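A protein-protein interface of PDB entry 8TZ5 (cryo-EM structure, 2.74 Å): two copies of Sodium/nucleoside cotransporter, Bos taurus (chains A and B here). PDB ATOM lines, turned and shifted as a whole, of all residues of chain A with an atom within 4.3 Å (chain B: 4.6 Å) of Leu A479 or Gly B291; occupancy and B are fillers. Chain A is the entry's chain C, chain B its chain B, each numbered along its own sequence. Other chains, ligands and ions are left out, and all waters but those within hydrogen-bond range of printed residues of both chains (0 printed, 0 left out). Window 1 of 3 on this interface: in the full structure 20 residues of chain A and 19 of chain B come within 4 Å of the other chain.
OG of Ser A483 sits at hydrogen-bond distance from O of Ala A480.
Among the printed residues, pairs that only touch across the chains: Ala A480 with Tyr B287 (3.3 Å), Ile A476 with Val B295 (3.3 Å), Ser A483 with Tyr B287 (3.5 Å), Leu A479 with Phe B294 (3.6 Å), Leu A475 with Phe B294 (3.7 Å), Leu A479 with Ala B290 (3.7 Å), Ile A476 with Gly B291 (3.7 Å), Leu A479 with Gly B291 (3.8 Å), Ala A480 with Ser B288 (3.8 Å) and Ser A483 with Ala B290 (3.97 Å).
Leu A479 touches just these residues of chain B: Ala B290 (3.7 Å), Gly B291 (3.8 Å) and Phe B294 (3.6 Å).
Of chain A, only Ile A476 and Leu A479 come within 4 Å of Gly B291.
Of the printed residues of chain A, Val B295 touches Ile A476 (3.3 Å).
Of the printed residues of chain A, Ala B290 touches Leu A479 and Ser A483.
No position is printed for both chains.
Of the 10 pairs that touch across the chains among the printed residues, none has its exchanged pair printed and touching as well.
Along chain B the printed residues that touch a printed residue of chain A span positions 287 to 295.
Of the 9 printed residues of chain A, 5 touch a printed residue of chain B.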
ATOM      1  N   LEU A 475      13.894  -2.371 -21.482  1.00  0.00           N
ATOM      2  CA  LEU A 475      13.813  -1.324 -22.492  1.00  0.00           C
ATOM      3  C   LEU A 475      12.556  -1.474 -23.336  1.00  0.00           C
ATOM      4  O   LEU A 475      11.859  -0.488 -23.605  1.00  0.00           O
ATOM      5  CB  LEU A 475      15.056  -1.351 -23.380  1.00  0.00           C
ATOM      6  CG  LEU A 475      16.296  -0.648 -22.831  1.00  0.00           C
ATOM      7  CD1 LEU A 475      17.516  -1.046 -23.633  1.00  0.00           C
ATOM      8  CD2 LEU A 475      16.108   0.860 -22.853  1.00  0.00           C
ATOM      9  N   ILE A 476      12.240  -2.703 -23.749  1.00  0.00           N
ATOM     10  CA  ILE A 476      11.033  -2.918 -24.545  1.00  0.00           C
ATOM     11  C   ILE A 476       9.807  -2.439 -23.778  1.00  0.00           C
ATOM     12  O   ILE A 476       8.984  -1.670 -24.294  1.00  0.00           O
ATOM     13  CB  ILE A 476      10.899  -4.400 -24.935  1.00  0.00           C
ATOM     14  CG1 ILE A 476      12.042  -4.815 -25.862  1.00  0.00           C
ATOM     15  CG2 ILE A 476       9.541  -4.642 -25.584  1.00  0.00           C
ATOM     16  CD1 ILE A 476      12.117  -6.303 -26.126  1.00  0.00           C
ATOM     17  N   ALA A 477       9.674  -2.887 -22.528  1.00  0.00           N
ATOM     18  CA  ALA A 477       8.489  -2.553 -21.747  1.00  0.00           C
ATOM     19  C   ALA A 477       8.394  -1.051 -21.504  1.00  0.00           C
ATOM     20  O   ALA A 477       7.319  -0.456 -21.635  1.00  0.00           O
ATOM     21  CB  ALA A 477       8.507  -3.315 -20.424  1.00  0.00           C
ATOM     22  N   PHE A 478       9.516  -0.418 -21.148  1.00  0.00           N
ATOM     23  CA  PHE A 478       9.502   1.011 -20.864  1.00  0.00           C
ATOM     24  C   PHE A 478       9.140   1.821 -22.100  1.00  0.00           C
ATOM     25  O   PHE A 478       8.372   2.783 -22.011  1.00  0.00           O
ATOM     26  CB  PHE A 478      10.862   1.452 -20.316  1.00  0.00           C
ATOM     27  CG  PHE A 478      11.112   1.055 -18.881  1.00  0.00           C
ATOM     28  CD1 PHE A 478      10.068   0.924 -17.977  1.00  0.00           C
ATOM     29  CD2 PHE A 478      12.403   0.823 -18.434  1.00  0.00           C
ATOM     30  CE1 PHE A 478      10.308   0.565 -16.666  1.00  0.00           C
ATOM     31  CE2 PHE A 478      12.645   0.465 -17.124  1.00  0.00           C
ATOM     32  CZ  PHE A 478      11.598   0.337 -16.240  1.00  0.00           C
ATOM     33  N   LEU A 479       9.681   1.457 -23.264  1.00  0.00           N
ATOM     34  CA  LEU A 479       9.367   2.225 -24.464  1.00  0.00           C
ATOM     35  C   LEU A 479       7.921   2.016 -24.899  1.00  0.00           C
ATOM     36  O   LEU A 479       7.267   2.967 -25.349  1.00  0.00           O
ATOM     37  CB  LEU A 479      10.336   1.857 -25.587  1.00  0.00           C
ATOM     38  CG  LEU A 479      11.800   2.218 -25.316  1.00  0.00           C
ATOM     39  CD1 LEU A 479      12.708   1.705 -26.421  1.00  0.00           C
ATOM     40  CD2 LEU A 479      11.969   3.719 -25.148  1.00  0.00           C
ATOM     41  N   ALA A 480       7.391   0.799 -24.745  1.00  0.00           N
ATOM     42  CA  ALA A 480       5.978   0.585 -25.033  1.00  0.00           C
ATOM     43  C   ALA A 480       5.096   1.405 -24.099  1.00  0.00           C
ATOM     44  O   ALA A 480       4.114   2.021 -24.537  1.00  0.00           O
ATOM     45  CB  ALA A 480       5.643  -0.901 -24.919  1.00  0.00           C
ATOM     46  N   LEU A 481       5.435   1.432 -22.807  1.00  0.00           N
ATOM     47  CA  LEU A 481       4.678   2.240 -21.858  1.00  0.00           C
ATOM     48  C   LEU A 481       4.762   3.719 -22.205  1.00  0.00           C
ATOM     49  O   LEU A 481       3.773   4.447 -22.085  1.00  0.00           O
ATOM     50  CB  LEU A 481       5.187   1.999 -20.439  1.00  0.00           C
ATOM     51  CG  LEU A 481       4.873   0.631 -19.838  1.00  0.00           C
ATOM     52  CD1 LEU A 481       5.637   0.431 -18.543  1.00  0.00           C
ATOM     53  CD2 LEU A 481       3.381   0.490 -19.607  1.00  0.00           C
ATOM     54  N   LEU A 482       5.942   4.186 -22.611  1.00  0.00           N
ATOM     55  CA  LEU A 482       6.092   5.587 -22.987  1.00  0.00           C
ATOM     56  C   LEU A 482       5.207   5.927 -24.180  1.00  0.00           C
ATOM     57  O   LEU A 482       4.530   6.962 -24.190  1.00  0.00           O
ATOM     58  CB  LEU A 482       7.559   5.888 -23.294  1.00  0.00           C
ATOM     59  CG  LEU A 482       7.868   7.320 -23.725  1.00  0.00           C
ATOM     60  CD1 LEU A 482       7.534   8.300 -22.612  1.00  0.00           C
ATOM     61  CD2 LEU A 482       9.320   7.440 -24.137  1.00  0.00           C
ATOM     62  N   SER A 483       5.197   5.063 -25.196  1.00  0.00           N
ATOM     63  CA  SER A 483       4.342   5.303 -26.355  1.00  0.00           C
ATOM     64  C   SER A 483       2.874   5.351 -25.947  1.00  0.00           C
ATOM     65  O   SER A 483       2.129   6.253 -26.354  1.00  0.00           O
ATOM     66  CB  SER A 483       4.568   4.219 -27.407  1.00  0.00           C
ATOM     67  OG  SER A 483       4.114   2.963 -26.939  1.00  0.00           O
ATOM     68  N   TYR B 287       1.652  -1.040 -29.245  1.00  0.00           N
ATOM     69  CA  TYR B 287       2.598  -0.224 -28.495  1.00  0.00           C
ATOM     70  C   TYR B 287       3.924  -0.934 -28.256  1.00  0.00           C
ATOM     71  O   TYR B 287       4.946  -0.264 -28.077  1.00  0.00           O
ATOM     72  CB  TYR B 287       1.974   0.185 -27.162  1.00  0.00           C
ATOM     73  CG  TYR B 287       0.766   1.085 -27.299  1.00  0.00           C
ATOM     74  CD1 TYR B 287       0.762   2.147 -28.193  1.00  0.00           C
ATOM     75  CD2 TYR B 287      -0.375   0.867 -26.542  1.00  0.00           C
ATOM     76  CE1 TYR B 287      -0.338   2.967 -28.322  1.00  0.00           C
ATOM     77  CE2 TYR B 287      -1.480   1.682 -26.666  1.00  0.00           C
ATOM     78  CZ  TYR B 287      -1.456   2.731 -27.557  1.00  0.00           C
ATOM     79  OH  TYR B 287      -2.555   3.546 -27.683  1.00  0.00           O
ATOM     80  N   SER B 288       3.932  -2.269 -28.243  1.00  0.00           N
ATOM     81  CA  SER B 288       5.178  -3.005 -28.061  1.00  0.00           C
ATOM     82  C   SER B 288       6.141  -2.798 -29.221  1.00  0.00           C
ATOM     83  O   SER B 288       7.344  -3.053 -29.072  1.00  0.00           O
ATOM     84  CB  SER B 288       4.882  -4.493 -27.889  1.00  0.00           C
ATOM     85  OG  SER B 288       4.142  -4.993 -28.987  1.00  0.00           O
ATOM     86  N   ASP B 289       5.637  -2.346 -30.371  1.00  0.00           N
ATOM     87  CA  ASP B 289       6.510  -2.073 -31.505  1.00  0.00           C
ATOM     88  C   ASP B 289       7.531  -0.997 -31.171  1.00  0.00           C
ATOM     89  O   ASP B 289       8.639  -1.007 -31.712  1.00  0.00           O
ATOM     90  CB  ASP B 289       5.674  -1.658 -32.715  1.00  0.00           C
ATOM     91  CG  ASP B 289       4.684  -2.726 -33.132  1.00  0.00           C
ATOM     92  OD1 ASP B 289       4.693  -3.816 -32.526  1.00  0.00           O
ATOM     93  OD2 ASP B 289       3.892  -2.471 -34.064  1.00  0.00           O
ATOM     94  N   ALA B 290       7.188  -0.076 -30.268  1.00  0.00           N
ATOM     95  CA  ALA B 290       8.122   0.984 -29.904  1.00  0.00           C
ATOM     96  C   ALA B 290       9.398   0.412 -29.299  1.00  0.00           C
ATOM     97  O   ALA B 290      10.504   0.844 -29.643  1.00  0.00           O
ATOM     98  CB  ALA B 290       7.454   1.951 -28.928  1.00  0.00           C
ATOM     99  N   GLY B 291       9.264  -0.548 -28.389  1.00  0.00           N
ATOM    100  CA  GLY B 291      10.416  -1.197 -27.799  1.00  0.00           C
ATOM    101  C   GLY B 291      11.071  -2.195 -28.728  1.00  0.00           C
ATOM    102  O   GLY B 291      12.300  -2.345 -28.733  1.00  0.00           O
ATOM    103  N   ALA B 292      10.253  -2.893 -29.522  1.00  0.00           N
ATOM    104  CA  ALA B 292      10.794  -3.891 -30.435  1.00  0.00           C
ATOM    105  C   ALA B 292      11.641  -3.256 -31.531  1.00  0.00           C
ATOM    106  O   ALA B 292      12.599  -3.874 -32.007  1.00  0.00           O
ATOM    107  CB  ALA B 292       9.658  -4.707 -31.049  1.00  0.00           C
ATOM    108  N   SER B 293      11.308  -2.031 -31.942  1.00  0.00           N
ATOM    109  CA  SER B 293      12.065  -1.344 -32.977  1.00  0.00           C
ATOM    110  C   SER B 293      13.382  -0.783 -32.466  1.00  0.00           C
ATOM    111  O   SER B 293      14.279  -0.519 -33.273  1.00  0.00           O
ATOM    112  CB  SER B 293      11.223  -0.211 -33.567  1.00  0.00           C
ATOM    113  OG  SER B 293      11.895   0.421 -34.641  1.00  0.00           O
ATOM    114  N   PHE B 294      13.520  -0.587 -31.156  1.00  0.00           N
ATOM    115  CA  PHE B 294      14.780  -0.122 -30.594  1.00  0.00           C
ATOM    116  C   PHE B 294      15.687  -1.282 -30.205  1.00  0.00           C
ATOM    117  O   PHE B 294      16.878  -1.276 -30.532  1.00  0.00           O
ATOM    118  CB  PHE B 294      14.526   0.774 -29.380  1.00  0.00           C
ATOM    119  CG  PHE B 294      15.775   1.131 -28.627  1.00  0.00           C
ATOM    120  CD1 PHE B 294      16.740   1.938 -29.208  1.00  0.00           C
ATOM    121  CD2 PHE B 294      15.989   0.656 -27.345  1.00  0.00           C
ATOM    122  CE1 PHE B 294      17.892   2.263 -28.523  1.00  0.00           C
ATOM    123  CE2 PHE B 294      17.140   0.980 -26.655  1.00  0.00           C
ATOM    124  CZ  PHE B 294      18.092   1.785 -27.244  1.00  0.00           C
ATOM    125  N   VAL B 295      15.146  -2.283 -29.509  1.00  0.00           N
ATOM    126  CA  VAL B 295      15.978  -3.406 -29.089  1.00  0.00           C
ATOM    127  C   VAL B 295      16.448  -4.209 -30.295  1.00  0.00           C
ATOM    128  O   VAL B 295      17.584  -4.696 -30.326  1.00  0.00           O
ATOM    129  CB  VAL B 295      15.223  -4.287 -28.080  1.00  0.00           C
ATOM    130  CG1 VAL B 295      16.010  -5.559 -27.798  1.00  0.00           C
ATOM    131  CG2 VAL B 295      14.968  -3.513 -26.798  1.00  0.00           C
